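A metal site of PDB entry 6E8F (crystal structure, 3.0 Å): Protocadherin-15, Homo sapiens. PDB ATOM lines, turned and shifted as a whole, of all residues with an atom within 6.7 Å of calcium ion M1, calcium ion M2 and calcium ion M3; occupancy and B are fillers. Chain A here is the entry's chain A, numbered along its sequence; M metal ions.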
ATOM      1  N   GLU A 145      -8.048   1.129 -24.814  1.00  0.00           N
ATOM      2  CA  GLU A 145      -9.075   0.663 -23.862  1.00  0.00           C
ATOM      3  C   GLU A 145      -8.587   0.942 -22.444  1.00  0.00           C
ATOM      4  O   GLU A 145      -9.382   1.099 -21.548  1.00  0.00           O
ATOM      5  CB  GLU A 145      -9.468  -0.797 -24.034  1.00  0.00           C
ATOM      6  CG  GLU A 145      -8.322  -1.775 -23.876  1.00  0.00           C
ATOM      7  CD  GLU A 145      -8.737  -3.231 -23.985  1.00  0.00           C
ATOM      8  OE1 GLU A 145      -9.891  -3.542 -23.643  1.00  0.00           O
ATOM      9  OE2 GLU A 145      -7.903  -4.063 -24.386  1.00  0.00           O
ATOM     10  N   VAL A 215     -13.772   2.275 -21.609  1.00  0.00           N
ATOM     11  CA  VAL A 215     -14.242   1.515 -22.748  1.00  0.00           C
ATOM     12  C   VAL A 215     -13.424   0.227 -22.874  1.00  0.00           C
ATOM     13  O   VAL A 215     -12.212   0.230 -22.737  1.00  0.00           O
ATOM     14  CB  VAL A 215     -14.165   2.355 -24.040  1.00  0.00           C
ATOM     15  CG1 VAL A 215     -15.235   3.439 -24.055  1.00  0.00           C
ATOM     16  CG2 VAL A 215     -12.771   2.941 -24.276  1.00  0.00           C
ATOM     17  N   ASP A 216     -14.130  -0.856 -23.175  1.00  0.00           N
ATOM     18  CA  ASP A 216     -13.592  -2.168 -23.224  1.00  0.00           C
ATOM     19  C   ASP A 216     -13.553  -2.609 -24.684  1.00  0.00           C
ATOM     20  O   ASP A 216     -14.604  -2.696 -25.334  1.00  0.00           O
ATOM     21  CB  ASP A 216     -14.464  -3.096 -22.378  1.00  0.00           C
ATOM     22  CG  ASP A 216     -13.912  -4.491 -22.162  1.00  0.00           C
ATOM     23  OD1 ASP A 216     -12.912  -4.860 -22.831  1.00  0.00           O
ATOM     24  OD2 ASP A 216     -14.525  -5.207 -21.346  1.00  0.00           O
ATOM     25  N   ARG A 217     -12.350  -2.884 -25.208  1.00  0.00           N
ATOM     26  CA  ARG A 217     -12.261  -3.311 -26.610  1.00  0.00           C
ATOM     27  C   ARG A 217     -13.007  -4.636 -26.791  1.00  0.00           C
ATOM     28  O   ARG A 217     -13.534  -4.927 -27.848  1.00  0.00           O
ATOM     29  CB  ARG A 217     -10.830  -3.486 -27.105  1.00  0.00           C
ATOM     30  CG  ARG A 217     -10.756  -3.739 -28.608  1.00  0.00           C
ATOM     31  CD  ARG A 217      -9.565  -4.595 -28.979  1.00  0.00           C
ATOM     32  NE  ARG A 217      -9.726  -5.938 -28.462  1.00  0.00           N
ATOM     33  CZ  ARG A 217     -10.323  -6.922 -29.133  1.00  0.00           C
ATOM     34  NH1 ARG A 217     -10.881  -6.660 -30.314  1.00  0.00           N
ATOM     35  NH2 ARG A 217     -10.336  -8.150 -28.642  1.00  0.00           N
ATOM     36  N   GLU A 218     -13.043  -5.444 -25.729  1.00  0.00           N
ATOM     37  CA  GLU A 218     -13.608  -6.769 -25.838  1.00  0.00           C
ATOM     38  C   GLU A 218     -15.142  -6.675 -25.890  1.00  0.00           C
ATOM     39  O   GLU A 218     -15.752  -7.548 -26.465  1.00  0.00           O
ATOM     40  CB  GLU A 218     -13.061  -7.667 -24.733  1.00  0.00           C
ATOM     41  CG  GLU A 218     -11.630  -8.131 -24.990  1.00  0.00           C
ATOM     42  CD  GLU A 218     -10.529  -7.072 -24.930  1.00  0.00           C
ATOM     43  OE1 GLU A 218     -10.486  -6.255 -23.935  1.00  0.00           O
ATOM     44  OE2 GLU A 218      -9.694  -7.071 -25.888  1.00  0.00           O
ATOM     45  N   GLU A 219     -15.752  -5.604 -25.335  1.00  0.00           N
ATOM     46  CA  GLU A 219     -17.189  -5.312 -25.595  1.00  0.00           C
ATOM     47  C   GLU A 219     -17.378  -4.784 -27.013  1.00  0.00           C
ATOM     48  O   GLU A 219     -17.743  -5.527 -27.924  1.00  0.00           O
ATOM     49  CB  GLU A 219     -17.749  -4.268 -24.628  1.00  0.00           C
ATOM     50  CG  GLU A 219     -18.385  -4.840 -23.388  1.00  0.00           C
ATOM     51  CD  GLU A 219     -18.483  -3.829 -22.265  1.00  0.00           C
ATOM     52  OE1 GLU A 219     -18.576  -4.258 -21.095  1.00  0.00           O
ATOM     53  OE2 GLU A 219     -18.429  -2.581 -22.567  1.00  0.00           O
ATOM     54  N   MET A 246      -8.370   0.724 -29.223  1.00  0.00           N
ATOM     55  CA  MET A 246      -7.172  -0.060 -29.471  1.00  0.00           C
ATOM     56  C   MET A 246      -6.924  -0.995 -28.288  1.00  0.00           C
ATOM     57  O   MET A 246      -7.159  -0.636 -27.111  1.00  0.00           O
ATOM     58  CB  MET A 246      -5.958   0.845 -29.657  1.00  0.00           C
ATOM     59  CG  MET A 246      -6.181   1.952 -30.657  1.00  0.00           C
ATOM     60  SD  MET A 246      -4.731   3.041 -30.782  1.00  0.00           S
ATOM     61  CE  MET A 246      -3.929   2.322 -32.213  1.00  0.00           C
ATOM     62  N   ASP A 247      -6.407  -2.188 -28.618  1.00  0.00           N
ATOM     63  CA  ASP A 247      -6.229  -3.284 -27.692  1.00  0.00           C
ATOM     64  C   ASP A 247      -5.123  -2.952 -26.697  1.00  0.00           C
ATOM     65  O   ASP A 247      -4.168  -2.247 -27.013  1.00  0.00           O
ATOM     66  CB  ASP A 247      -5.895  -4.573 -28.432  1.00  0.00           C
ATOM     67  CG  ASP A 247      -6.028  -5.819 -27.564  1.00  0.00           C
ATOM     68  OD1 ASP A 247      -7.148  -6.102 -27.082  1.00  0.00           O
ATOM     69  OD2 ASP A 247      -5.006  -6.492 -27.379  1.00  0.00           O
ATOM     70  N   ALA A 248      -5.312  -3.437 -25.468  1.00  0.00           N
ATOM     71  CA  ALA A 248      -4.317  -3.577 -24.454  1.00  0.00           C
ATOM     72  C   ALA A 248      -4.348  -5.029 -24.001  1.00  0.00           C
ATOM     73  O   ALA A 248      -5.361  -5.721 -24.217  1.00  0.00           O
ATOM     74  CB  ALA A 248      -4.632  -2.647 -23.325  1.00  0.00           C
ATOM     75  N   ASN A 249      -3.260  -5.496 -23.370  1.00  0.00           N
ATOM     76  CA  ASN A 249      -3.180  -6.856 -22.860  1.00  0.00           C
ATOM     77  C   ASN A 249      -3.795  -6.893 -21.456  1.00  0.00           C
ATOM     78  O   ASN A 249      -3.069  -6.978 -20.458  1.00  0.00           O
ATOM     79  CB  ASN A 249      -1.768  -7.427 -22.888  1.00  0.00           C
ATOM     80  CG  ASN A 249      -1.775  -8.938 -22.753  1.00  0.00           C
ATOM     81  OD1 ASN A 249      -2.737  -9.581 -23.165  1.00  0.00           O
ATOM     82  ND2 ASN A 249      -0.728  -9.514 -22.192  1.00  0.00           N
ATOM     83  N   ASP A 250      -5.134  -6.857 -21.397  1.00  0.00           N
ATOM     84  CA  ASP A 250      -5.891  -6.912 -20.139  1.00  0.00           C
ATOM     85  C   ASP A 250      -6.570  -8.273 -19.956  1.00  0.00           C
ATOM     86  O   ASP A 250      -7.463  -8.424 -19.122  1.00  0.00           O
ATOM     87  CB  ASP A 250      -6.909  -5.768 -20.025  1.00  0.00           C
ATOM     88  CG  ASP A 250      -7.750  -5.437 -21.261  1.00  0.00           C
ATOM     89  OD1 ASP A 250      -7.894  -6.309 -22.148  1.00  0.00           O
ATOM     90  OD2 ASP A 250      -8.273  -4.304 -21.309  1.00  0.00           O
ATOM     91  N   ASN A 251      -6.169  -9.298 -20.731  1.00  0.00           N
ATOM     92  CA  ASN A 251      -6.800 -10.596 -20.621  1.00  0.00           C
ATOM     93  C   ASN A 251      -5.734 -11.693 -20.586  1.00  0.00           C
ATOM     94  O   ASN A 251      -4.915 -11.823 -21.504  1.00  0.00           O
ATOM     95  CB  ASN A 251      -7.812 -10.814 -21.742  1.00  0.00           C
ATOM     96  CG  ASN A 251      -9.053  -9.974 -21.524  1.00  0.00           C
ATOM     97  OD1 ASN A 251      -9.973 -10.407 -20.824  1.00  0.00           O
ATOM     98  ND2 ASN A 251      -9.069  -8.770 -22.076  1.00  0.00           N
ATOM     99  N   THR A 252      -5.782 -12.466 -19.492  1.00  0.00           N
ATOM    100  CA  THR A 252      -4.854 -13.548 -19.234  1.00  0.00           C
ATOM    101  C   THR A 252      -5.324 -14.776 -20.014  1.00  0.00           C
ATOM    102  O   THR A 252      -6.527 -14.988 -20.170  1.00  0.00           O
ATOM    103  CB  THR A 252      -4.781 -13.832 -17.734  1.00  0.00           C
ATOM    104  OG1 THR A 252      -4.463 -12.626 -17.036  1.00  0.00           O
ATOM    105  CG2 THR A 252      -3.727 -14.871 -17.409  1.00  0.00           C
ATOM    106  N   PRO A 253      -4.402 -15.599 -20.566  1.00  0.00           N
ATOM    107  CA  PRO A 253      -4.791 -16.864 -21.198  1.00  0.00           C
ATOM    108  C   PRO A 253      -5.215 -17.762 -20.037  1.00  0.00           C
ATOM    109  O   PRO A 253      -4.366 -18.135 -19.264  1.00  0.00           O
ATOM    110  CB  PRO A 253      -3.549 -17.372 -21.939  1.00  0.00           C
ATOM    111  CG  PRO A 253      -2.588 -16.186 -21.915  1.00  0.00           C
ATOM    112  CD  PRO A 253      -2.958 -15.360 -20.701  1.00  0.00           C
ATOM    113  N   ASP A 281      -7.749 -16.480 -24.700  1.00  0.00           N
ATOM    114  CA  ASP A 281      -7.307 -15.126 -24.416  1.00  0.00           C
ATOM    115  C   ASP A 281      -8.125 -14.224 -25.319  1.00  0.00           C
ATOM    116  O   ASP A 281      -7.885 -14.213 -26.521  1.00  0.00           O
ATOM    117  CB  ASP A 281      -5.816 -14.918 -24.701  1.00  0.00           C
ATOM    118  CG  ASP A 281      -5.236 -13.618 -24.160  1.00  0.00           C
ATOM    119  OD1 ASP A 281      -5.928 -12.574 -24.212  1.00  0.00           O
ATOM    120  OD2 ASP A 281      -4.084 -13.646 -23.692  1.00  0.00           O
ATOM    121  N   ALA A 282      -9.053 -13.473 -24.726  1.00  0.00           N
ATOM    122  CA  ALA A 282     -10.019 -12.659 -25.476  1.00  0.00           C
ATOM    123  C   ALA A 282      -9.344 -11.498 -26.234  1.00  0.00           C
ATOM    124  O   ALA A 282      -9.949 -10.932 -27.117  1.00  0.00           O
ATOM    125  CB  ALA A 282     -11.069 -12.141 -24.531  1.00  0.00           C
ATOM    126  N   ASP A 283      -8.091 -11.149 -25.884  1.00  0.00           N
ATOM    127  CA  ASP A 283      -7.369 -10.036 -26.501  1.00  0.00           C
ATOM    128  C   ASP A 283      -7.249 -10.221 -28.019  1.00  0.00           C
ATOM    129  O   ASP A 283      -7.551 -11.282 -28.565  1.00  0.00           O
ATOM    130  CB  ASP A 283      -6.011  -9.843 -25.840  1.00  0.00           C
ATOM    131  CG  ASP A 283      -6.091  -9.264 -24.430  1.00  0.00           C
ATOM    132  OD1 ASP A 283      -7.044  -8.489 -24.173  1.00  0.00           O
ATOM    133  OD2 ASP A 283      -5.206  -9.596 -23.608  1.00  0.00           O
ATOM    134  N   GLU A 284      -6.811  -9.141 -28.670  1.00  0.00           N
ATOM    135  CA  GLU A 284      -6.686  -9.021 -30.119  1.00  0.00           C
ATOM    136  C   GLU A 284      -5.214  -9.172 -30.487  1.00  0.00           C
ATOM    137  O   GLU A 284      -4.297  -8.891 -29.688  1.00  0.00           O
ATOM    138  CB  GLU A 284      -7.236  -7.659 -30.588  1.00  0.00           C
ATOM    139  CG  GLU A 284      -6.685  -7.153 -31.931  1.00  0.00           C
ATOM    140  CD  GLU A 284      -7.240  -5.827 -32.451  1.00  0.00           C
ATOM    141  OE1 GLU A 284      -6.941  -4.774 -31.852  1.00  0.00           O
ATOM    142  OE2 GLU A 284      -7.961  -5.855 -33.472  1.00  0.00           O
ATOM    143  N   SER A 286      -1.575 -10.183 -31.201  1.00  0.00           N
ATOM    144  CA  SER A 286      -0.686 -11.115 -30.504  1.00  0.00           C
ATOM    145  C   SER A 286      -0.842 -10.998 -28.973  1.00  0.00           C
ATOM    146  O   SER A 286      -0.342 -11.810 -28.231  1.00  0.00           O
ATOM    147  CB  SER A 286       0.728 -10.937 -30.961  1.00  0.00           C
ATOM    148  OG  SER A 286       1.330  -9.895 -30.240  1.00  0.00           O
ATOM    149  N   ASN A 287      -1.625 -10.020 -28.501  1.00  0.00           N
ATOM    150  CA  ASN A 287      -1.997  -9.954 -27.088  1.00  0.00           C
ATOM    151  C   ASN A 287      -2.913 -11.118 -26.713  1.00  0.00           C
ATOM    152  O   ASN A 287      -3.072 -11.419 -25.509  1.00  0.00           O
ATOM    153  CB  ASN A 287      -2.704  -8.644 -26.749  1.00  0.00           C
ATOM    154  CG  ASN A 287      -1.795  -7.443 -26.882  1.00  0.00           C
ATOM    155  OD1 ASN A 287      -0.830  -7.478 -27.637  1.00  0.00           O
ATOM    156  ND2 ASN A 287      -2.078  -6.398 -26.131  1.00  0.00           N
ATOM    157  N   GLY A 288      -3.534 -11.743 -27.725  1.00  0.00           N
ATOM    158  CA  GLY A 288      -4.464 -12.850 -27.553  1.00  0.00           C
ATOM    159  C   GLY A 288      -3.972 -14.131 -28.195  1.00  0.00           C
ATOM    160  O   GLY A 288      -4.692 -15.123 -28.210  1.00  0.00           O
ATOM    161  N   GLU A 289      -2.744 -14.096 -28.717  1.00  0.00           N
ATOM    162  CA  GLU A 289      -2.027 -15.251 -29.273  1.00  0.00           C
ATOM    163  C   GLU A 289      -1.418 -16.026 -28.101  1.00  0.00           C
ATOM    164  O   GLU A 289      -0.804 -15.420 -27.241  1.00  0.00           O
ATOM    165  CB  GLU A 289      -0.964 -14.717 -30.237  1.00  0.00           C
ATOM    166  CG  GLU A 289      -0.554 -15.640 -31.365  1.00  0.00           C
ATOM    167  CD  GLU A 289       0.885 -15.372 -31.808  1.00  0.00           C
ATOM    168  OE1 GLU A 289       1.805 -15.798 -31.076  1.00  0.00           O
ATOM    169  OE2 GLU A 289       1.086 -14.680 -32.824  1.00  0.00           O
ATOM    170  N   ASP A 333       0.405 -15.355 -23.328  1.00  0.00           N
ATOM    171  CA  ASP A 333       0.143 -14.608 -24.569  1.00  0.00           C
ATOM    172  C   ASP A 333       1.467 -14.075 -25.120  1.00  0.00           C
ATOM    173  O   ASP A 333       2.470 -14.074 -24.398  1.00  0.00           O
ATOM    174  CB  ASP A 333      -0.904 -13.508 -24.352  1.00  0.00           C
ATOM    175  CG  ASP A 333      -0.594 -12.488 -23.267  1.00  0.00           C
ATOM    176  OD1 ASP A 333       0.605 -12.230 -22.993  1.00  0.00           O
ATOM    177  OD2 ASP A 333      -1.549 -11.926 -22.706  1.00  0.00           O
ATOM    178  N   ASN A 334       1.478 -13.626 -26.381  1.00  0.00           N
ATOM    179  CA  ASN A 334       2.692 -13.123 -27.046  1.00  0.00           C
ATOM    180  C   ASN A 334       2.721 -11.588 -27.048  1.00  0.00           C
ATOM    181  O   ASN A 334       3.123 -10.980 -28.034  1.00  0.00           O
ATOM    182  CB  ASN A 334       2.879 -13.713 -28.449  1.00  0.00           C
ATOM    183  CG  ASN A 334       3.133 -15.214 -28.412  1.00  0.00           C
ATOM    184  OD1 ASN A 334       2.595 -15.910 -27.560  1.00  0.00           O
ATOM    185  ND2 ASN A 334       3.966 -15.714 -29.311  1.00  0.00           N
ATOM    186  N   ALA A 335       2.359 -10.972 -25.923  1.00  0.00           N
ATOM    187  CA  ALA A 335       2.585  -9.530 -25.748  1.00  0.00           C
ATOM    188  C   ALA A 335       4.080  -9.301 -25.598  1.00  0.00           C
ATOM    189  O   ALA A 335       4.843 -10.253 -25.452  1.00  0.00           O
ATOM    190  CB  ALA A 335       1.828  -9.017 -24.549  1.00  0.00           C
ATOM    191  N   GLU A 339       4.589  -6.620 -20.532  1.00  0.00           N
ATOM    192  CA  GLU A 339       3.113  -6.493 -20.468  1.00  0.00           C
ATOM    193  C   GLU A 339       2.425  -7.861 -20.667  1.00  0.00           C
ATOM    194  O   GLU A 339       1.200  -7.909 -20.847  1.00  0.00           O
ATOM    195  CB  GLU A 339       2.624  -5.558 -21.586  1.00  0.00           C
ATOM    196  CG  GLU A 339       3.264  -4.183 -21.564  1.00  0.00           C
ATOM    197  CD  GLU A 339       3.578  -3.630 -22.953  1.00  0.00           C
ATOM    198  OE1 GLU A 339       2.873  -4.010 -23.918  1.00  0.00           O
ATOM    199  OE2 GLU A 339       4.552  -2.852 -23.078  1.00  0.00           O
ATOM    200  N   ARG A 341       1.096 -11.817 -20.068  1.00  0.00           N
ATOM    201  CA  ARG A 341       0.387 -12.493 -18.996  1.00  0.00           C
ATOM    202  C   ARG A 341       0.353 -13.990 -19.261  1.00  0.00           C
ATOM    203  O   ARG A 341       0.519 -14.431 -20.396  1.00  0.00           O
ATOM    204  CB  ARG A 341      -1.042 -11.985 -18.858  1.00  0.00           C
ATOM    205  CG  ARG A 341      -1.130 -10.579 -18.294  1.00  0.00           C
ATOM    206  CD  ARG A 341      -2.029  -9.679 -19.123  1.00  0.00           C
ATOM    207  NE  ARG A 341      -2.470  -8.561 -18.304  1.00  0.00           N
ATOM    208  CZ  ARG A 341      -3.375  -8.662 -17.340  1.00  0.00           C
ATOM    209  NH1 ARG A 341      -3.978  -9.820 -17.138  1.00  0.00           N
ATOM    210  NH2 ARG A 341      -3.651  -7.621 -16.601  1.00  0.00           N
HETATM  211 CA    CA M   1      -7.814  -6.220 -24.804  1.00  0.00          CA
HETATM  212 CA    CA M   2     -10.719  -4.937 -21.756  1.00  0.00          CA
HETATM  213 CA    CA M   3      -3.673 -11.429 -23.287  1.00  0.00          CA
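The side-chain amide nitrogen of Asn 249 lies within hydrogen-bond range of the backbone carbonyl oxygen of Glu 339 (2.8 Å). OE1 of Glu 145 sits close to N of Arg 217 (3.0 Å). N of Glu 145 lies within hydrogen-bond range of O of Met 246, at 3.0 Å. The side-chain amide nitrogen (ND2) of Asn 251 lies close to the side-chain carboxylate (OE1) of Glu 218 (3.4 Å). ND2 of Asn 251 sits close to OD1 of Asp 250, 2.7 Å away. The backbone NH (N) of Arg 341 is in hydrogen-bond range of the side-chain carboxylate (OD1) of Asp 333, 3.0 Å away. The side-chain carboxylate (OE2) of Glu 218 sits close to the guanidinium group (NE) of Arg 217 (2.8 Å). The side-chain carboxylate of Asp 247 lies close to the guanidinium group of Arg 217, at 2.9 Å.
The nearest printed residue that does not touch calcium ion M1 is Arg 217 (4.1 Å).
Four residues have an atom within 4 Å of calcium ion M2: Glu 145, Asp 216, Glu 218 and Asp 250. The nearest printed residue that does not touch calcium ion M2 is Asn 251 (4.2 Å).
Of the 27 residues printed, 6 come within 4 Å of calcium ion M3. The nearest printed residue that does not touch calcium ion M3 is Gly 288 (4.5 Å).
Calcium ion M1 is bound by OE2 of Glu 145 (2.2 Å), OE2 of Glu 218 (2.3 Å), OD1 of Asp 247 (2.4 Å), OD1 of Asp 283 (2.5 Å), O of Ala 248 (2.6 Å), OD1 of Asp 250 (2.7 Å) and OE1 of Glu 218 (2.8 Å).
Calcium ion M2 is bound by OD1 of Asp 216 (2.4 Å), OE1 of Glu 145 (2.5 Å), OE1 of Glu 218 (2.6 Å) and OD2 of Asp 250 (2.6 Å). Calcium ion M2 has four donor atoms within binding distance.
Calcium ion M3 is bound by the side-chain amide oxygen (OD1) of Asn 249, the backbone carbonyl oxygen (O) of Asn 251, the side-chain carboxylate (OD2) of Asp 333, the side-chain carboxylate (OD2) of Asp 281, the backbone carbonyl oxygen (O) of Asn 287, the side-chain carboxylate (OD2) of Asp 283 and the side-chain carboxylate (OD1) of Asp 281.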
